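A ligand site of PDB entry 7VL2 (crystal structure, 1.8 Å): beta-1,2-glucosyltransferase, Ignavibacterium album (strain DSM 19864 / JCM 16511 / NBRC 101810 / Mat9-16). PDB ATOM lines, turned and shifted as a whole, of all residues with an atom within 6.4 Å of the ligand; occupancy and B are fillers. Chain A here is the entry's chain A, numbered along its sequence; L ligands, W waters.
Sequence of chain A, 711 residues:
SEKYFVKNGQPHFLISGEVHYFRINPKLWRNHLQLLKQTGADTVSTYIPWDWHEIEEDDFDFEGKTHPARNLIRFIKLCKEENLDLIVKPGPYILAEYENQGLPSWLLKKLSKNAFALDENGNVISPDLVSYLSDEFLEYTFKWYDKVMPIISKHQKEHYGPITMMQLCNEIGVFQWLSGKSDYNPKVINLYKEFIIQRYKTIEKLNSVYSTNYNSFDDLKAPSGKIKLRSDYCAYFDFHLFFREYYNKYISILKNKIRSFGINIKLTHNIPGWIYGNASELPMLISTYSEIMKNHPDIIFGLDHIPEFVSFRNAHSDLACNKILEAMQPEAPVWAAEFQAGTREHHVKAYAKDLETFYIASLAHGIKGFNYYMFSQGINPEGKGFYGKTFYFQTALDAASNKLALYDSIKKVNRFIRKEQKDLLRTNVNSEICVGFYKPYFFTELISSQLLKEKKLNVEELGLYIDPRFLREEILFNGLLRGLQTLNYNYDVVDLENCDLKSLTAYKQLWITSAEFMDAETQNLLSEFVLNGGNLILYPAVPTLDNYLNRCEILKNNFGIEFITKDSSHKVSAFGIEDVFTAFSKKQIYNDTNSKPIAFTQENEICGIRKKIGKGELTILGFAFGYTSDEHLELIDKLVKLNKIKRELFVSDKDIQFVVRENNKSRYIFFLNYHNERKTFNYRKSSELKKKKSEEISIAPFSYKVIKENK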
ATOM      1  N   LEU A  95     -12.198   3.873   9.042  1.00  0.00           N
ATOM      2  CA  LEU A  95     -11.495   5.172   9.139  1.00  0.00           C
ATOM      3  C   LEU A  95     -12.526   6.276   8.847  1.00  0.00           C
ATOM      4  O   LEU A  95     -13.319   6.564   9.753  1.00  0.00           O
ATOM      5  CB  LEU A  95     -10.289   5.211   8.193  1.00  0.00           C
ATOM      6  CG  LEU A  95      -8.996   4.565   8.699  1.00  0.00           C
ATOM      7  CD1 LEU A  95      -8.446   5.336   9.869  1.00  0.00           C
ATOM      8  CD2 LEU A  95      -9.171   3.093   9.096  1.00  0.00           C
ATOM      9  N   ALA A  96     -12.589   6.772   7.616  1.00  0.00           N
ATOM     10  CA  ALA A  96     -13.697   7.641   7.139  1.00  0.00           C
ATOM     11  C   ALA A  96     -13.878   8.880   8.034  1.00  0.00           C
ATOM     12  O   ALA A  96     -14.998   9.448   8.019  1.00  0.00           O
ATOM     13  CB  ALA A  96     -14.973   6.855   7.122  1.00  0.00           C
ATOM     14  N   GLU A  97     -12.848   9.320   8.782  1.00  0.00           N
ATOM     15  CA  GLU A  97     -12.983  10.460   9.755  1.00  0.00           C
ATOM     16  C   GLU A  97     -14.250  10.263  10.598  1.00  0.00           C
ATOM     17  O   GLU A  97     -14.951  11.237  10.882  1.00  0.00           O
ATOM     18  CB  GLU A  97     -13.012  11.785   8.966  1.00  0.00           C
ATOM     19  CG  GLU A  97     -11.930  11.872   7.879  1.00  0.00           C
ATOM     20  CD  GLU A  97     -10.944  13.020   7.967  1.00  0.00           C
ATOM     21  OE1 GLU A  97     -11.317  14.083   8.496  1.00  0.00           O
ATOM     22  OE2 GLU A  97      -9.777  12.865   7.487  1.00  0.00           O
ATOM     23  N   GLN A 101     -12.655   5.473  14.284  1.00  0.00           N
ATOM     24  CA  GLN A 101     -12.324   4.852  12.977  1.00  0.00           C
ATOM     25  C   GLN A 101     -13.434   3.860  12.605  1.00  0.00           C
ATOM     26  O   GLN A 101     -13.163   2.937  11.777  1.00  0.00           O
ATOM     27  CB  GLN A 101     -10.940   4.192  13.060  1.00  0.00           C
ATOM     28  CG  GLN A 101      -9.880   5.077  13.715  1.00  0.00           C
ATOM     29  CD  GLN A 101      -9.554   6.278  12.875  1.00  0.00           C
ATOM     30  OE1 GLN A 101     -10.102   6.490  11.798  1.00  0.00           O
ATOM     31  NE2 GLN A 101      -8.615   7.080  13.338  1.00  0.00           N
ATOM     32  N   ASN A 170     -10.152  -1.647   5.984  1.00  0.00           N
ATOM     33  CA  ASN A 170      -9.810  -0.362   5.335  1.00  0.00           C
ATOM     34  C   ASN A 170      -8.316  -0.078   5.551  1.00  0.00           C
ATOM     35  O   ASN A 170      -7.934  -0.003   6.714  1.00  0.00           O
ATOM     36  CB  ASN A 170     -10.673   0.794   5.864  1.00  0.00           C
ATOM     37  CG  ASN A 170     -10.562   2.052   5.042  1.00  0.00           C
ATOM     38  OD1 ASN A 170     -11.279   2.225   4.046  1.00  0.00           O
ATOM     39  ND2 ASN A 170      -9.620   2.912   5.405  1.00  0.00           N
ATOM     40  N   GLU A 171      -7.547   0.033   4.477  1.00  0.00           N
ATOM     41  CA  GLU A 171      -6.115   0.465   4.520  1.00  0.00           C
ATOM     42  C   GLU A 171      -5.355  -0.291   5.620  1.00  0.00           C
ATOM     43  O   GLU A 171      -4.828   0.317   6.539  1.00  0.00           O
ATOM     44  CB  GLU A 171      -6.059   1.966   4.725  1.00  0.00           C
ATOM     45  CG  GLU A 171      -6.601   2.732   3.531  1.00  0.00           C
ATOM     46  CD  GLU A 171      -6.517   4.234   3.673  1.00  0.00           C
ATOM     47  OE1 GLU A 171      -6.386   4.727   4.796  1.00  0.00           O
ATOM     48  OE2 GLU A 171      -6.548   4.925   2.627  1.00  0.00           O
ATOM     49  N   VAL A 174      -2.501   1.057   8.132  1.00  0.00           N
ATOM     50  CA  VAL A 174      -2.390   2.553   8.047  1.00  0.00           C
ATOM     51  C   VAL A 174      -2.101   3.147   9.452  1.00  0.00           C
ATOM     52  O   VAL A 174      -1.588   4.271   9.505  1.00  0.00           O
ATOM     53  CB  VAL A 174      -3.606   3.197   7.339  1.00  0.00           C
ATOM     54  CG1 VAL A 174      -4.876   3.237   8.176  1.00  0.00           C
ATOM     55  CG2 VAL A 174      -3.264   4.583   6.803  1.00  0.00           C
ATOM     56  N   PHE A 175      -2.357   2.433  10.558  1.00  0.00           N
ATOM     57  CA  PHE A 175      -2.024   2.908  11.939  1.00  0.00           C
ATOM     58  C   PHE A 175      -0.636   2.471  12.407  1.00  0.00           C
ATOM     59  O   PHE A 175       0.065   3.301  12.997  1.00  0.00           O
ATOM     60  CB  PHE A 175      -3.069   2.436  12.930  1.00  0.00           C
ATOM     61  CG  PHE A 175      -4.484   2.737  12.514  1.00  0.00           C
ATOM     62  CD1 PHE A 175      -4.928   4.044  12.489  1.00  0.00           C
ATOM     63  CD2 PHE A 175      -5.377   1.707  12.227  1.00  0.00           C
ATOM     64  CE1 PHE A 175      -6.239   4.321  12.129  1.00  0.00           C
ATOM     65  CE2 PHE A 175      -6.685   1.977  11.888  1.00  0.00           C
ATOM     66  CZ  PHE A 175      -7.109   3.285  11.836  1.00  0.00           C
ATOM     67  N   TRP A 177       1.578   2.587  10.489  1.00  0.00           N
ATOM     68  CA  TRP A 177       2.250   3.661   9.719  1.00  0.00           C
ATOM     69  C   TRP A 177       2.043   5.036  10.394  1.00  0.00           C
ATOM     70  O   TRP A 177       3.062   5.656  10.712  1.00  0.00           O
ATOM     71  CB  TRP A 177       1.787   3.611   8.252  1.00  0.00           C
ATOM     72  CG  TRP A 177       2.339   4.714   7.412  1.00  0.00           C
ATOM     73  CD1 TRP A 177       3.655   5.037   7.224  1.00  0.00           C
ATOM     74  CD2 TRP A 177       1.575   5.624   6.589  1.00  0.00           C
ATOM     75  NE1 TRP A 177       3.758   6.079   6.347  1.00  0.00           N
ATOM     76  CE2 TRP A 177       2.501   6.479   5.949  1.00  0.00           C
ATOM     77  CE3 TRP A 177       0.215   5.811   6.349  1.00  0.00           C
ATOM     78  CZ2 TRP A 177       2.103   7.497   5.098  1.00  0.00           C
ATOM     79  CZ3 TRP A 177      -0.190   6.822   5.497  1.00  0.00           C
ATOM     80  CH2 TRP A 177       0.755   7.654   4.884  1.00  0.00           C
ATOM     81  N   LEU A 178       0.822   5.528  10.604  1.00  0.00           N
ATOM     82  CA  LEU A 178       0.565   6.952  10.987  1.00  0.00           C
ATOM     83  C   LEU A 178       0.853   7.186  12.477  1.00  0.00           C
ATOM     84  O   LEU A 178       1.325   8.308  12.805  1.00  0.00           O
ATOM     85  CB  LEU A 178      -0.875   7.379  10.678  1.00  0.00           C
ATOM     86  CG  LEU A 178      -1.208   7.661   9.219  1.00  0.00           C
ATOM     87  CD1 LEU A 178      -2.601   8.237   9.118  1.00  0.00           C
ATOM     88  CD2 LEU A 178      -0.232   8.613   8.553  1.00  0.00           C
ATOM     89  N   ASN A 270      -7.859  -1.293  -0.238  1.00  0.00           N
ATOM     90  CA  ASN A 270      -7.537   0.098  -0.640  1.00  0.00           C
ATOM     91  C   ASN A 270      -6.177   0.476  -0.066  1.00  0.00           C
ATOM     92  O   ASN A 270      -5.902   0.130   1.087  1.00  0.00           O
ATOM     93  CB  ASN A 270      -8.633   1.057  -0.247  1.00  0.00           C
ATOM     94  CG  ASN A 270      -9.025   1.031   1.211  1.00  0.00           C
ATOM     95  OD1 ASN A 270      -8.962  -0.012   1.874  1.00  0.00           O
ATOM     96  ND2 ASN A 270      -9.536   2.165   1.673  1.00  0.00           N
ATOM     97  N   ILE A 271      -5.361   1.111  -0.885  1.00  0.00           N
ATOM     98  CA  ILE A 271      -3.944   1.402  -0.553  1.00  0.00           C
ATOM     99  C   ILE A 271      -3.814   2.860  -0.126  1.00  0.00           C
ATOM    100  O   ILE A 271      -4.060   3.771  -0.934  1.00  0.00           O
ATOM    101  CB  ILE A 271      -3.067   1.112  -1.767  1.00  0.00           C
ATOM    102  CG1 ILE A 271      -3.251  -0.318  -2.295  1.00  0.00           C
ATOM    103  CG2 ILE A 271      -1.623   1.389  -1.420  1.00  0.00           C
ATOM    104  CD1 ILE A 271      -2.888  -0.419  -3.736  1.00  0.00           C
ATOM    105  N   PRO A 272      -3.349   3.075   1.126  1.00  0.00           N
ATOM    106  CA  PRO A 272      -3.029   4.416   1.604  1.00  0.00           C
ATOM    107  C   PRO A 272      -1.607   4.831   1.158  1.00  0.00           C
ATOM    108  O   PRO A 272      -0.873   4.027   0.627  1.00  0.00           O
ATOM    109  CB  PRO A 272      -3.037   4.189   3.120  1.00  0.00           C
ATOM    110  CG  PRO A 272      -2.479   2.802   3.295  1.00  0.00           C
ATOM    111  CD  PRO A 272      -2.980   2.033   2.093  1.00  0.00           C
ATOM    112  N   GLY A 273      -1.216   6.077   1.438  1.00  0.00           N
ATOM    113  CA  GLY A 273       0.183   6.510   1.285  1.00  0.00           C
ATOM    114  C   GLY A 273       0.357   7.959   0.929  1.00  0.00           C
ATOM    115  O   GLY A 273       1.480   8.469   1.042  1.00  0.00           O
ATOM    116  N   TRP A 274      -0.671   8.612   0.409  1.00  0.00           N
ATOM    117  CA  TRP A 274      -0.501  10.045   0.086  1.00  0.00           C
ATOM    118  C   TRP A 274      -0.533  10.815   1.401  1.00  0.00           C
ATOM    119  O   TRP A 274      -1.389  10.512   2.258  1.00  0.00           O
ATOM    120  CB  TRP A 274      -1.589  10.574  -0.847  1.00  0.00           C
ATOM    121  CG  TRP A 274      -1.556  10.112  -2.259  1.00  0.00           C
ATOM    122  CD1 TRP A 274      -1.914   8.888  -2.734  1.00  0.00           C
ATOM    123  CD2 TRP A 274      -1.223  10.911  -3.391  1.00  0.00           C
ATOM    124  NE1 TRP A 274      -1.821   8.866  -4.087  1.00  0.00           N
ATOM    125  CE2 TRP A 274      -1.429  10.106  -4.530  1.00  0.00           C
ATOM    126  CE3 TRP A 274      -0.780  12.229  -3.571  1.00  0.00           C
ATOM    127  CZ2 TRP A 274      -1.183  10.564  -5.826  1.00  0.00           C
ATOM    128  CZ3 TRP A 274      -0.541  12.689  -4.845  1.00  0.00           C
ATOM    129  CH2 TRP A 274      -0.724  11.856  -5.950  1.00  0.00           C
ATOM    130  N   ILE A 275       0.299  11.856   1.505  1.00  0.00           N
ATOM    131  CA  ILE A 275       0.138  12.828   2.606  1.00  0.00           C
ATOM    132  C   ILE A 275       0.735  14.146   2.132  1.00  0.00           C
ATOM    133  O   ILE A 275       1.754  14.120   1.420  1.00  0.00           O
ATOM    134  CB  ILE A 275       0.772  12.263   3.890  1.00  0.00           C
ATOM    135  CG1 ILE A 275       0.329  13.026   5.141  1.00  0.00           C
ATOM    136  CG2 ILE A 275       2.271  12.167   3.716  1.00  0.00           C
ATOM    137  CD1 ILE A 275       0.843  12.413   6.452  1.00  0.00           C
ATOM    138  N   TYR A 276       0.055  15.237   2.425  1.00  0.00           N
ATOM    139  CA  TYR A 276       0.511  16.586   2.029  1.00  0.00           C
ATOM    140  C   TYR A 276       0.616  16.699   0.500  1.00  0.00           C
ATOM    141  O   TYR A 276       1.365  17.543   0.045  1.00  0.00           O
ATOM    142  CB  TYR A 276       1.829  16.934   2.739  1.00  0.00           C
ATOM    143  CG  TYR A 276       1.833  16.658   4.235  1.00  0.00           C
ATOM    144  CD1 TYR A 276       0.818  17.124   5.073  1.00  0.00           C
ATOM    145  CD2 TYR A 276       2.854  15.932   4.816  1.00  0.00           C
ATOM    146  CE1 TYR A 276       0.820  16.861   6.449  1.00  0.00           C
ATOM    147  CE2 TYR A 276       2.865  15.637   6.174  1.00  0.00           C
ATOM    148  CZ  TYR A 276       1.844  16.097   6.997  1.00  0.00           C
ATOM    149  OH  TYR A 276       1.881  15.769   8.325  1.00  0.00           O
ATOM    150  N   ASP A 304      -5.801   4.929  -3.173  1.00  0.00           N
ATOM    151  CA  ASP A 304      -6.443   6.068  -2.471  1.00  0.00           C
ATOM    152  C   ASP A 304      -5.652   7.322  -2.836  1.00  0.00           C
ATOM    153  O   ASP A 304      -4.680   7.606  -2.135  1.00  0.00           O
ATOM    154  CB  ASP A 304      -6.519   5.768  -0.970  1.00  0.00           C
ATOM    155  CG  ASP A 304      -7.420   4.585  -0.662  1.00  0.00           C
ATOM    156  OD1 ASP A 304      -8.163   4.149  -1.585  1.00  0.00           O
ATOM    157  OD2 ASP A 304      -7.464   4.173   0.506  1.00  0.00           O
ATOM    158  N   ILE A 306      -4.847  11.134  -3.135  1.00  0.00           N
ATOM    159  CA  ILE A 306      -5.107  12.429  -2.432  1.00  0.00           C
ATOM    160  C   ILE A 306      -4.055  13.466  -2.845  1.00  0.00           C
ATOM    161  O   ILE A 306      -3.272  13.938  -2.007  1.00  0.00           O
ATOM    162  CB  ILE A 306      -5.197  12.301  -0.897  1.00  0.00           C
ATOM    163  CG1 ILE A 306      -5.970  11.064  -0.427  1.00  0.00           C
ATOM    164  CG2 ILE A 306      -5.816  13.587  -0.353  1.00  0.00           C
ATOM    165  CD1 ILE A 306      -5.837  10.824   1.055  1.00  0.00           C
ATOM    166  N   GLU A 308      -4.430  16.756  -3.549  1.00  0.00           N
ATOM    167  CA  GLU A 308      -4.728  18.063  -2.869  1.00  0.00           C
ATOM    168  C   GLU A 308      -4.565  19.258  -3.823  1.00  0.00           C
ATOM    169  O   GLU A 308      -5.246  20.248  -3.643  1.00  0.00           O
ATOM    170  CB  GLU A 308      -3.858  18.292  -1.632  1.00  0.00           C
ATOM    171  CG  GLU A 308      -3.942  17.171  -0.584  1.00  0.00           C
ATOM    172  CD  GLU A 308      -3.192  17.360   0.717  1.00  0.00           C
ATOM    173  OE1 GLU A 308      -2.433  18.353   0.845  1.00  0.00           O
ATOM    174  OE2 GLU A 308      -3.396  16.542   1.628  1.00  0.00           O
ATOM    175  N   GLU A 338     -10.388   5.296  -3.944  1.00  0.00           N
ATOM    176  CA  GLU A 338     -10.737   6.625  -3.415  1.00  0.00           C
ATOM    177  C   GLU A 338     -10.004   7.613  -4.312  1.00  0.00           C
ATOM    178  O   GLU A 338      -8.764   7.554  -4.367  1.00  0.00           O
ATOM    179  CB  GLU A 338     -10.328   6.750  -1.936  1.00  0.00           C
ATOM    180  CG  GLU A 338     -10.933   5.692  -1.009  1.00  0.00           C
ATOM    181  CD  GLU A 338     -10.421   5.775   0.409  1.00  0.00           C
ATOM    182  OE1 GLU A 338      -9.837   6.798   0.784  1.00  0.00           O
ATOM    183  OE2 GLU A 338     -10.586   4.806   1.141  1.00  0.00           O
ATOM    184  N   ARG A 344     -11.001  16.482   2.464  1.00  0.00           N
ATOM    185  CA  ARG A 344     -11.259  16.017   3.850  1.00  0.00           C
ATOM    186  C   ARG A 344     -11.015  17.109   4.892  1.00  0.00           C
ATOM    187  O   ARG A 344     -11.553  16.965   6.031  1.00  0.00           O
ATOM    188  CB  ARG A 344     -10.378  14.792   4.129  1.00  0.00           C
ATOM    189  CG  ARG A 344      -8.894  15.107   4.027  1.00  0.00           C
ATOM    190  CD  ARG A 344      -8.100  13.832   4.207  1.00  0.00           C
ATOM    191  NE  ARG A 344      -6.693  14.076   3.996  1.00  0.00           N
ATOM    192  CZ  ARG A 344      -5.762  13.178   4.262  1.00  0.00           C
ATOM    193  NH1 ARG A 344      -4.481  13.482   4.127  1.00  0.00           N
ATOM    194  NH2 ARG A 344      -6.141  11.995   4.714  1.00  0.00           N
HETATM  195  C1  LIG L   1      -5.799   8.792   5.819  1.00  0.00           C
HETATM  196  C2  LIG L   1      -6.080   8.217   4.423  1.00  0.00           C
HETATM  197  O1  LIG L   1      -7.050   7.186   4.494  1.00  0.00           O
HETATM  198  C3  LIG L   1      -4.806   7.649   3.794  1.00  0.00           C
HETATM  199  O2  LIG L   1      -5.090   7.247   2.441  1.00  0.00           O
HETATM  200  C4  LIG L   1      -3.685   8.716   3.811  1.00  0.00           C
HETATM  201  O3  LIG L   1      -2.509   8.145   3.245  1.00  0.00           O
HETATM  202  C5  LIG L   1      -3.453   9.131   5.269  1.00  0.00           C
HETATM  203  O4  LIG L   1      -4.660   9.670   5.800  1.00  0.00           O
HETATM  204  C6  LIG L   1      -2.394  10.221   5.391  1.00  0.00           C
HETATM  205  O5  LIG L   1      -2.699  11.363   4.520  1.00  0.00           O
HETATM  206  O6  LIG L   1      -5.504   7.742   6.757  1.00  0.00           O
HETATM  207  C7  LIG L   1      -5.904   8.120   8.086  1.00  0.00           C
HETATM  208  C8  LIG L   1      -5.404   7.033   9.016  1.00  0.00           C
HETATM  209  O   HOH W   1      -9.315   5.122   3.466  1.00  0.00           O
HETATM  210  O   HOH W   2      -3.596   8.009   0.271  1.00  0.00           O
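Merely in contact with the ligand: Leu 95, Val 174, Trp 177, Leu 178, Pro 272, Ile 275, Asp 304 and Ile 306.
Hydrophobic or aromatic side chains that line the ligand: Leu 95, Val 174, Trp 177, Leu 178, Pro 272, Ile 275 and Ile 306.
Within 4 Å of the ligand: Leu 95, Glu 171, Val 174, Trp 177, Leu 178, Pro 272, Gly 273, Trp 274, Ile 275, Asp 304, Ile 306 and Arg 344.
O3 of the ligand lies within hydrogen-bond range of N of Trp 274.
N of Gly 273 lies within hydrogen-bond range of O3 of the ligand (3.0 Å).
The backbone carbonyl oxygen (O) of Trp 274 sits at hydrogen-bond distance from an oxygen (O5) of the ligand (2.7 Å).
OE1 of Glu 171 is in hydrogen-bond range of O1 of the ligand.
O5 of the ligand is in hydrogen-bond range of NH1 of Arg 344, 2.8 Å away.
The backbone NH (N) of Leu 95 is in hydrogen-bond range of the backbone carbonyl oxygen (O) of Gln 101, at 3.0 Å.
The backbone NH (N) of Glu 171 lies within hydrogen-bond range of the side-chain amide oxygen (OD1) of Asn 270 (3.0 Å).
The side-chain carboxylate (OD1) of Asp 304 lies close to the backbone NH (N) of Glu 338.
The side-chain carboxylate (OD2) of Asp 304 sits at hydrogen-bond distance from the side-chain amide nitrogen (ND2) of Asn 270.
The side-chain carboxylate (OE2) of Glu 171 lies close to the side-chain carboxylate (OD2) of Asp 304.
The backbone NH of Asp 304 sits at hydrogen-bond distance from the backbone carbonyl oxygen of Ile 271 (3.1 Å).
Water W2 lies within hydrogen-bond range of O of Asp 304 (2.7 Å), O2 of the ligand (2.7 Å), N of Trp 274 (3.0 Å) and N of Gly 273 (3.3 Å).
Water W1 lies within hydrogen-bond range of the side-chain carboxylate of Glu 338 (2.7 Å), the side-chain carboxylate of Glu 171 (2.9 Å), the side-chain amide nitrogen of Asn 170 (3.0 Å), an oxygen (O1) of the ligand (3.2 Å) and the side-chain amide nitrogen of Asn 270 (3.5 Å).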
